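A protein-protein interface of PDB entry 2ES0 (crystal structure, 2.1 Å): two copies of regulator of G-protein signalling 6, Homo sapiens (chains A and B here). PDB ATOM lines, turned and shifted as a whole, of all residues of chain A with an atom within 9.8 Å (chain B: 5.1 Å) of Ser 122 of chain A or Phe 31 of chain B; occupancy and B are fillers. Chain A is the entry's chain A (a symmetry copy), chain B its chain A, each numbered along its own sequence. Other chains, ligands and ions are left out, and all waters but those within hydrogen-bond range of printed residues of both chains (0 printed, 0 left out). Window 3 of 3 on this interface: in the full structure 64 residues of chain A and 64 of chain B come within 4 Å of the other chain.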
ATOM      1  N   MET A 111      15.633  -1.100  26.407  1.00  0.00           N
ATOM      2  CA  MET A 111      16.347  -2.388  26.442  1.00  0.00           C
ATOM      3  C   MET A 111      15.672  -3.394  27.380  1.00  0.00           C
ATOM      4  O   MET A 111      15.542  -4.572  27.045  1.00  0.00           O
ATOM      5  CB  MET A 111      17.798  -2.182  26.887  1.00  0.00           C
ATOM      6  CG  MET A 111      18.664  -1.457  25.873  1.00  0.00           C
ATOM      7  SD  MET A 111      20.388  -1.499  26.355  1.00  0.00           S
ATOM      8  CE  MET A 111      20.381  -0.349  27.745  1.00  0.00           C
ATOM      9  N   LYS A 112      15.254  -2.917  28.553  1.00  0.00           N
ATOM     10  CA  LYS A 112      14.625  -3.773  29.556  1.00  0.00           C
ATOM     11  C   LYS A 112      13.307  -4.350  29.047  1.00  0.00           C
ATOM     12  O   LYS A 112      13.070  -5.558  29.152  1.00  0.00           O
ATOM     13  CB  LYS A 112      14.390  -3.014  30.872  1.00  0.00           C
ATOM     14  CG  LYS A 112      14.010  -3.951  32.028  1.00  0.00           C
ATOM     15  CD  LYS A 112      13.331  -3.251  33.203  1.00  0.00           C
ATOM     16  CE  LYS A 112      14.325  -2.512  34.076  1.00  0.00           C
ATOM     17  NZ  LYS A 112      13.773  -2.166  35.433  1.00  0.00           N
ATOM     18  N   SER A 113      12.454  -3.488  28.492  1.00  0.00           N
ATOM     19  CA  SER A 113      11.148  -3.925  28.006  1.00  0.00           C
ATOM     20  C   SER A 113      11.221  -4.659  26.662  1.00  0.00           C
ATOM     21  O   SER A 113      10.521  -5.647  26.473  1.00  0.00           O
ATOM     22  CB  SER A 113      10.180  -2.741  27.911  1.00  0.00           C
ATOM     23  OG  SER A 113      10.654  -1.759  27.009  1.00  0.00           O
ATOM     24  N   ASP A 114      12.061  -4.192  25.731  1.00  0.00           N
ATOM     25  CA  ASP A 114      11.976  -4.667  24.334  1.00  0.00           C
ATOM     26  C   ASP A 114      13.045  -5.665  23.893  1.00  0.00           C
ATOM     27  O   ASP A 114      12.838  -6.372  22.909  1.00  0.00           O
ATOM     28  CB  ASP A 114      11.960  -3.484  23.355  1.00  0.00           C
ATOM     29  CG  ASP A 114      10.646  -2.685  23.399  1.00  0.00           C
ATOM     30  OD1 ASP A 114       9.812  -2.891  24.315  1.00  0.00           O
ATOM     31  OD2 ASP A 114      10.451  -1.838  22.499  1.00  0.00           O
ATOM     32  N   SER A 115      14.177  -5.716  24.590  1.00  0.00           N
ATOM     33  CA  SER A 115      15.295  -6.591  24.201  1.00  0.00           C
ATOM     34  C   SER A 115      15.620  -7.680  25.222  1.00  0.00           C
ATOM     35  O   SER A 115      15.998  -8.788  24.849  1.00  0.00           O
ATOM     36  CB  SER A 115      16.556  -5.757  23.976  1.00  0.00           C
ATOM     37  OG  SER A 115      16.357  -4.786  22.971  1.00  0.00           O
ATOM     38  N   TYR A 116      15.494  -7.353  26.505  1.00  0.00           N
ATOM     39  CA  TYR A 116      15.922  -8.253  27.580  1.00  0.00           C
ATOM     40  C   TYR A 116      15.192  -9.598  27.559  1.00  0.00           C
ATOM     41  O   TYR A 116      15.841 -10.638  27.478  1.00  0.00           O
ATOM     42  CB  TYR A 116      15.806  -7.568  28.951  1.00  0.00           C
ATOM     43  CG  TYR A 116      16.104  -8.485  30.124  1.00  0.00           C
ATOM     44  CD1 TYR A 116      17.303  -9.196  30.194  1.00  0.00           C
ATOM     45  CD2 TYR A 116      15.185  -8.644  31.161  1.00  0.00           C
ATOM     46  CE1 TYR A 116      17.577 -10.041  31.274  1.00  0.00           C
ATOM     47  CE2 TYR A 116      15.450  -9.486  32.237  1.00  0.00           C
ATOM     48  CZ  TYR A 116      16.643 -10.178  32.287  1.00  0.00           C
ATOM     49  OH  TYR A 116      16.898 -11.010  33.352  1.00  0.00           O
ATOM     50  N   ALA A 117      13.859  -9.588  27.610  1.00  0.00           N
ATOM     51  CA  ALA A 117      13.080 -10.842  27.569  1.00  0.00           C
ATOM     52  C   ALA A 117      13.347 -11.666  26.312  1.00  0.00           C
ATOM     53  O   ALA A 117      13.372 -12.896  26.363  1.00  0.00           O
ATOM     54  CB  ALA A 117      11.591 -10.565  27.701  1.00  0.00           C
ATOM     55  N   ARG A 118      13.548 -10.987  25.185  1.00  0.00           N
ATOM     56  CA  ARG A 118      13.870 -11.665  23.930  1.00  0.00           C
ATOM     57  C   ARG A 118      15.206 -12.399  24.005  1.00  0.00           C
ATOM     58  O   ARG A 118      15.323 -13.531  23.520  1.00  0.00           O
ATOM     59  CB  ARG A 118      13.921 -10.661  22.777  1.00  0.00           C
ATOM     60  CG  ARG A 118      12.565 -10.157  22.315  1.00  0.00           C
ATOM     61  CD  ARG A 118      12.713  -9.264  21.086  1.00  0.00           C
ATOM     62  NE  ARG A 118      13.455  -9.937  20.022  1.00  0.00           N
ATOM     63  CZ  ARG A 118      12.970 -10.915  19.265  1.00  0.00           C
ATOM     64  NH1 ARG A 118      11.729 -11.354  19.425  1.00  0.00           N
ATOM     65  NH2 ARG A 118      13.734 -11.459  18.325  1.00  0.00           N
ATOM     66  N   PHE A 119      16.214 -11.744  24.586  1.00  0.00           N
ATOM     67  CA  PHE A 119      17.516 -12.373  24.828  1.00  0.00           C
ATOM     68  C   PHE A 119      17.349 -13.706  25.553  1.00  0.00           C
ATOM     69  O   PHE A 119      17.884 -14.727  25.127  1.00  0.00           O
ATOM     70  CB  PHE A 119      18.425 -11.454  25.651  1.00  0.00           C
ATOM     71  CG  PHE A 119      19.747 -12.073  26.015  1.00  0.00           C
ATOM     72  CD1 PHE A 119      20.145 -12.168  27.339  1.00  0.00           C
ATOM     73  CD2 PHE A 119      20.593 -12.567  25.031  1.00  0.00           C
ATOM     74  CE1 PHE A 119      21.369 -12.740  27.675  1.00  0.00           C
ATOM     75  CE2 PHE A 119      21.814 -13.146  25.362  1.00  0.00           C
ATOM     76  CZ  PHE A 119      22.201 -13.229  26.685  1.00  0.00           C
ATOM     77  N   LEU A 120      16.586 -13.684  26.637  1.00  0.00           N
ATOM     78  CA  LEU A 120      16.390 -14.864  27.458  1.00  0.00           C
ATOM     79  C   LEU A 120      15.766 -16.014  26.670  1.00  0.00           C
ATOM     80  O   LEU A 120      16.087 -17.180  26.909  1.00  0.00           O
ATOM     81  CB  LEU A 120      15.528 -14.517  28.668  1.00  0.00           C
ATOM     82  CG  LEU A 120      16.129 -13.477  29.607  1.00  0.00           C
ATOM     83  CD1 LEU A 120      15.201 -13.260  30.796  1.00  0.00           C
ATOM     84  CD2 LEU A 120      17.535 -13.886  30.057  1.00  0.00           C
ATOM     85  N   ARG A 121      14.901 -15.684  25.714  1.00  0.00           N
ATOM     86  CA  ARG A 121      14.288 -16.696  24.855  1.00  0.00           C
ATOM     87  C   ARG A 121      15.222 -17.122  23.726  1.00  0.00           C
ATOM     88  O   ARG A 121      14.932 -18.072  23.022  1.00  0.00           O
ATOM     89  CB  ARG A 121      12.963 -16.194  24.265  1.00  0.00           C
ATOM     90  CG  ARG A 121      11.993 -15.593  25.292  1.00  0.00           C
ATOM     91  CD  ARG A 121      10.534 -15.494  24.783  1.00  0.00           C
ATOM     92  NE  ARG A 121       9.998 -14.136  24.941  1.00  0.00           N
ATOM     93  CZ  ARG A 121       9.913 -13.221  23.968  1.00  0.00           C
ATOM     94  NH1 ARG A 121      10.285 -13.502  22.717  1.00  0.00           N
ATOM     95  NH2 ARG A 121       9.435 -12.010  24.247  1.00  0.00           N
ATOM     96  N   SER A 122      16.341 -16.433  23.545  1.00  0.00           N
ATOM     97  CA  SER A 122      17.190 -16.698  22.384  1.00  0.00           C
ATOM     98  C   SER A 122      17.923 -18.018  22.535  1.00  0.00           C
ATOM     99  O   SER A 122      18.224 -18.456  23.645  1.00  0.00           O
ATOM    100  CB  SER A 122      18.203 -15.566  22.153  1.00  0.00           C
ATOM    101  OG  SER A 122      19.231 -15.571  23.125  1.00  0.00           O
ATOM    102  N   ASN A 123      18.206 -18.649  21.405  1.00  0.00           N
ATOM    103  CA  ASN A 123      19.088 -19.807  21.395  1.00  0.00           C
ATOM    104  C   ASN A 123      20.483 -19.415  21.865  1.00  0.00           C
ATOM    105  O   ASN A 123      21.133 -20.175  22.570  1.00  0.00           O
ATOM    106  CB  ASN A 123      19.130 -20.437  20.006  1.00  0.00           C
ATOM    107  CG  ASN A 123      17.805 -21.060  19.621  1.00  0.00           C
ATOM    108  OD1 ASN A 123      17.253 -21.871  20.367  1.00  0.00           O
ATOM    109  ND2 ASN A 123      17.282 -20.681  18.462  1.00  0.00           N
ATOM    110  N   ALA A 124      20.924 -18.214  21.500  1.00  0.00           N
ATOM    111  CA  ALA A 124      22.182 -17.676  22.013  1.00  0.00           C
ATOM    112  C   ALA A 124      22.284 -17.900  23.522  1.00  0.00           C
ATOM    113  O   ALA A 124      23.255 -18.498  23.993  1.00  0.00           O
ATOM    114  CB  ALA A 124      22.311 -16.180  21.682  1.00  0.00           C
ATOM    115  N   TYR A 125      21.267 -17.449  24.259  1.00  0.00           N
ATOM    116  CA  TYR A 125      21.233 -17.589  25.719  1.00  0.00           C
ATOM    117  C   TYR A 125      20.993 -19.035  26.162  1.00  0.00           C
ATOM    118  O   TYR A 125      21.792 -19.596  26.914  1.00  0.00           O
ATOM    119  CB  TYR A 125      20.151 -16.690  26.327  1.00  0.00           C
ATOM    120  CG  TYR A 125      20.021 -16.824  27.830  1.00  0.00           C
ATOM    121  CD1 TYR A 125      20.945 -16.231  28.684  1.00  0.00           C
ATOM    122  CD2 TYR A 125      18.979 -17.554  28.398  1.00  0.00           C
ATOM    123  CE1 TYR A 125      20.832 -16.353  30.064  1.00  0.00           C
ATOM    124  CE2 TYR A 125      18.855 -17.683  29.777  1.00  0.00           C
ATOM    125  CZ  TYR A 125      19.783 -17.081  30.605  1.00  0.00           C
ATOM    126  OH  TYR A 125      19.664 -17.206  31.970  1.00  0.00           O
ATOM    127  N   GLN A 126      19.893 -19.620  25.696  1.00  0.00           N
ATOM    128  CA  GLN A 126      19.468 -20.962  26.131  1.00  0.00           C
ATOM    129  C   GLN A 126      20.542 -22.028  25.895  1.00  0.00           C
ATOM    130  O   GLN A 126      20.681 -22.950  26.694  1.00  0.00           O
ATOM    131  CB  GLN A 126      18.161 -21.370  25.437  1.00  0.00           C
ATOM    132  CG  GLN A 126      16.947 -20.514  25.811  1.00  0.00           C
ATOM    133  CD  GLN A 126      16.473 -20.723  27.244  1.00  0.00           C
ATOM    134  OE1 GLN A 126      16.452 -21.847  27.747  1.00  0.00           O
ATOM    135  NE2 GLN A 126      16.071 -19.638  27.900  1.00  0.00           N
ATOM    136  N   ASP A 127      21.303 -21.889  24.810  1.00  0.00           N
ATOM    137  CA  ASP A 127      22.427 -22.792  24.521  1.00  0.00           C
ATOM    138  C   ASP A 127      23.508 -22.758  25.613  1.00  0.00           C
ATOM    139  O   ASP A 127      24.209 -23.750  25.821  1.00  0.00           O
ATOM    140  CB  ASP A 127      23.063 -22.470  23.156  1.00  0.00           C
ATOM    141  CG  ASP A 127      22.135 -22.776  21.977  1.00  0.00           C
ATOM    142  OD1 ASP A 127      21.350 -23.750  22.053  1.00  0.00           O
ATOM    143  OD2 ASP A 127      22.200 -22.039  20.964  1.00  0.00           O
ATOM    144  N   LEU A 128      23.639 -21.623  26.302  1.00  0.00           N
ATOM    145  CA  LEU A 128      24.563 -21.508  27.437  1.00  0.00           C
ATOM    146  C   LEU A 128      24.066 -22.292  28.653  1.00  0.00           C
ATOM    147  O   LEU A 128      24.870 -22.818  29.425  1.00  0.00           O
ATOM    148  CB  LEU A 128      24.767 -20.045  27.844  1.00  0.00           C
ATOM    149  CG  LEU A 128      25.124 -19.035  26.755  1.00  0.00           C
ATOM    150  CD1 LEU A 128      25.266 -17.646  27.359  1.00  0.00           C
ATOM    151  CD2 LEU A 128      26.392 -19.435  26.021  1.00  0.00           C
ATOM    152  N   LEU A 129      22.744 -22.370  28.820  1.00  0.00           N
ATOM    153  CA  LEU A 129      22.151 -22.984  30.019  1.00  0.00           C
ATOM    154  C   LEU A 129      22.345 -24.500  30.140  1.00  0.00           C
ATOM    155  O   LEU A 129      21.877 -25.096  31.108  1.00  0.00           O
ATOM    156  CB  LEU A 129      20.660 -22.618  30.167  1.00  0.00           C
ATOM    157  CG  LEU A 129      20.341 -21.409  31.058  1.00  0.00           C
ATOM    158  CD1 LEU A 129      18.831 -21.265  31.209  1.00  0.00           C
ATOM    159  CD2 LEU A 129      20.997 -21.520  32.436  1.00  0.00           C
ATOM    160  N   GLN B  27      27.536 -10.920  26.114  1.00  0.00           N
ATOM    161  CA  GLN B  27      26.656 -11.880  25.459  1.00  0.00           C
ATOM    162  C   GLN B  27      25.407 -11.165  24.965  1.00  0.00           C
ATOM    163  O   GLN B  27      24.970 -11.377  23.833  1.00  0.00           O
ATOM    164  CB  GLN B  27      26.255 -13.018  26.402  1.00  0.00           C
ATOM    165  CG  GLN B  27      27.268 -14.161  26.505  1.00  0.00           C
ATOM    166  CD  GLN B  27      27.563 -14.809  25.163  1.00  0.00           C
ATOM    167  OE1 GLN B  27      26.676 -15.377  24.521  1.00  0.00           O
ATOM    168  NE2 GLN B  27      28.816 -14.711  24.724  1.00  0.00           N
ATOM    169  N   PHE B  28      24.848 -10.326  25.837  1.00  0.00           N
ATOM    170  CA  PHE B  28      23.693  -9.498  25.510  1.00  0.00           C
ATOM    171  C   PHE B  28      23.998  -8.617  24.306  1.00  0.00           C
ATOM    172  O   PHE B  28      23.160  -8.465  23.431  1.00  0.00           O
ATOM    173  CB  PHE B  28      23.292  -8.640  26.720  1.00  0.00           C
ATOM    174  CG  PHE B  28      21.995  -7.881  26.542  1.00  0.00           C
ATOM    175  CD1 PHE B  28      20.826  -8.539  26.170  1.00  0.00           C
ATOM    176  CD2 PHE B  28      21.934  -6.508  26.782  1.00  0.00           C
ATOM    177  CE1 PHE B  28      19.628  -7.847  26.018  1.00  0.00           C
ATOM    178  CE2 PHE B  28      20.727  -5.809  26.629  1.00  0.00           C
ATOM    179  CZ  PHE B  28      19.583  -6.479  26.247  1.00  0.00           C
ATOM    180  N   LEU B  29      25.212  -8.066  24.265  1.00  0.00           N
ATOM    181  CA  LEU B  29      25.633  -7.190  23.185  1.00  0.00           C
ATOM    182  C   LEU B  29      25.673  -7.921  21.845  1.00  0.00           C
ATOM    183  O   LEU B  29      25.258  -7.370  20.828  1.00  0.00           O
ATOM    184  CB  LEU B  29      27.006  -6.583  23.489  1.00  0.00           C
ATOM    185  CG  LEU B  29      27.582  -5.633  22.435  1.00  0.00           C
ATOM    186  CD1 LEU B  29      26.719  -4.387  22.291  1.00  0.00           C
ATOM    187  CD2 LEU B  29      29.022  -5.252  22.753  1.00  0.00           C
ATOM    188  N   ARG B  30      26.189  -9.148  21.844  1.00  0.00           N
ATOM    189  CA  ARG B  30      26.219  -9.962  20.619  1.00  0.00           C
ATOM    190  C   ARG B  30      24.795 -10.266  20.137  1.00  0.00           C
ATOM    191  O   ARG B  30      24.535 -10.295  18.936  1.00  0.00           O
ATOM    192  CB  ARG B  30      27.026 -11.250  20.838  1.00  0.00           C
ATOM    193  CG  ARG B  30      28.527 -10.986  21.054  1.00  0.00           C
ATOM    194  CD  ARG B  30      29.286 -12.239  21.483  1.00  0.00           C
ATOM    195  NE  ARG B  30      30.629 -11.928  21.979  1.00  0.00           N
ATOM    196  N   PHE B  31      23.879 -10.466  21.081  1.00  0.00           N
ATOM    197  CA  PHE B  31      22.459 -10.618  20.766  1.00  0.00           C
ATOM    198  C   PHE B  31      21.882  -9.345  20.157  1.00  0.00           C
ATOM    199  O   PHE B  31      21.180  -9.399  19.149  1.00  0.00           O
ATOM    200  CB  PHE B  31      21.661 -10.994  22.014  1.00  0.00           C
ATOM    201  CG  PHE B  31      20.170 -11.069  21.781  1.00  0.00           C
ATOM    202  CD1 PHE B  31      19.625 -12.108  21.033  1.00  0.00           C
ATOM    203  CD2 PHE B  31      19.321 -10.106  22.311  1.00  0.00           C
ATOM    204  CE1 PHE B  31      18.253 -12.187  20.815  1.00  0.00           C
ATOM    205  CE2 PHE B  31      17.952 -10.170  22.095  1.00  0.00           C
ATOM    206  CZ  PHE B  31      17.415 -11.213  21.345  1.00  0.00           C
ATOM    207  N   LEU B  32      22.162  -8.197  20.769  1.00  0.00           N
ATOM    208  CA  LEU B  32      21.671  -6.935  20.228  1.00  0.00           C
ATOM    209  C   LEU B  32      22.237  -6.693  18.829  1.00  0.00           C
ATOM    210  O   LEU B  32      21.547  -6.174  17.968  1.00  0.00           O
ATOM    211  CB  LEU B  32      22.008  -5.762  21.157  1.00  0.00           C
ATOM    212  CG  LEU B  32      21.414  -5.771  22.571  1.00  0.00           C
ATOM    213  CD1 LEU B  32      21.658  -4.431  23.261  1.00  0.00           C
ATOM    214  CD2 LEU B  32      19.916  -6.118  22.567  1.00  0.00           C
ATOM    215  N   GLU B  33      23.485  -7.087  18.596  1.00  0.00           N
ATOM    216  CA  GLU B  33      24.067  -6.959  17.262  1.00  0.00           C
ATOM    217  C   GLU B  33      23.298  -7.756  16.203  1.00  0.00           C
ATOM    218  O   GLU B  33      23.082  -7.259  15.099  1.00  0.00           O
ATOM    219  CB  GLU B  33      25.544  -7.347  17.272  1.00  0.00           C
ATOM    220  CG  GLU B  33      26.416  -6.277  17.900  1.00  0.00           C
ATOM    221  CD  GLU B  33      27.841  -6.727  18.129  1.00  0.00           C
ATOM    222  OE1 GLU B  33      28.105  -7.952  18.081  1.00  0.00           O
ATOM    223  OE2 GLU B  33      28.704  -5.847  18.357  1.00  0.00           O
ATOM    224  N   SER B  34      22.859  -8.968  16.549  1.00  0.00           N
ATOM    225  CA  SER B  34      22.022  -9.771  15.649  1.00  0.00           C
ATOM    226  C   SER B  34      20.613  -9.191  15.504  1.00  0.00           C
ATOM    227  O   SER B  34      19.934  -9.471  14.529  1.00  0.00           O
ATOM    228  CB  SER B  34      21.941 -11.220  16.133  1.00  0.00           C
ATOM    229  OG  SER B  34      21.190 -11.331  17.331  1.00  0.00           O
ATOM    230  N   GLU B  35      20.182  -8.399  16.485  1.00  0.00           N
ATOM    231  CA  GLU B  35      18.905  -7.679  16.444  1.00  0.00           C
ATOM    232  C   GLU B  35      19.007  -6.312  15.769  1.00  0.00           C
ATOM    233  O   GLU B  35      17.996  -5.636  15.599  1.00  0.00           O
ATOM    234  CB  GLU B  35      18.412  -7.432  17.871  1.00  0.00           C
ATOM    235  CG  GLU B  35      18.153  -8.683  18.684  1.00  0.00           C
ATOM    236  CD  GLU B  35      16.707  -9.098  18.651  1.00  0.00           C
ATOM    237  OE1 GLU B  35      15.878  -8.385  19.262  1.00  0.00           O
ATOM    238  OE2 GLU B  35      16.402 -10.129  18.011  1.00  0.00           O
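Ser 122 of chain A touches one residue of chain B. Phe 31 of chain B touches four residues of chain A. No residue of chain A comes within 4 Å of Ser 34 of chain B. Printed residues of chain A within 4 Å of Leu 32 of chain B: Ser 115 (3.7 Å). Of the printed residues of chain B, Phe 119 of chain A touches Gln 27 (3.9 Å), Phe 28 (3.7 Å) and Phe 31 (3.4 Å). Of the printed residues of chain B, Arg 118 of chain A touches Phe 31 (3.7 Å) and Glu 35 (3.0 Å). Leu 29 of chain B touches none of the printed residues of chain A. Gln 126 of chain A touches none of the printed residues of chain B. The nearest residue of chain A that does not touch Phe 31 of chain B is Ala 124 of chain A (4.9 Å). The nearest printed residue of chain B that does not touch Phe 119 of chain A is Leu 29 of chain B (6.2 Å).
OE1 of Glu 35 of chain B is in salt-bridge range of NE of Arg 118 of chain A, 3.0 Å away.
CB of Ser 115 of chain A touches CZ of Phe 28 of chain B (3.9 Å). Ser 115 of chain A touches Phe 31 of chain B (O to CE2, 3.6 Å). Ser 115 of chain A touches Leu 32 of chain B (CB to CD2, 3.7 Å). Arg 118 of chain A touches Phe 31 of chain B. O of Gln 27 of chain B touches CE2 of Phe 119 of chain A (3.9 Å). Phe 119 of chain A touches Phe 28 of chain B. N of Phe 119 of chain A touches CE2 of Phe 31 of chain B (3.4 Å). Ser 122 of chain A touches Phe 31 of chain B (CB to CE1, 3.6 Å). Gln 27 of chain B touches Leu 128 of chain A (OE1 to CD1, 3.9 Å).
No position is printed for both chains. Of the 10 pairs that touch across the chains among the printed residues, none has its exchanged pair printed and touching as well.
Hydrophobic or aromatic side chains of chain B within 4 Å of the printed part of chain A: Phe 28, Phe 31 and Leu 32. Of the 19 printed residues of chain A, 5 touch a printed residue of chain B. Among the printed residues, 10 pairs touch across the chains.
O of Phe 119 of chain A sits at hydrogen-bond distance from OG of Ser 122 of chain A (2.6 Å). The side-chain hydroxyl (OG) of Ser 122 of chain A is in hydrogen-bond range of the backbone NH (N) of Tyr 125 of chain A, 3.0 Å away. The side-chain hydroxyl of Ser 34 of chain B sits at hydrogen-bond distance from the backbone carbonyl oxygen of Phe 31 of chain B (2.7 Å).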
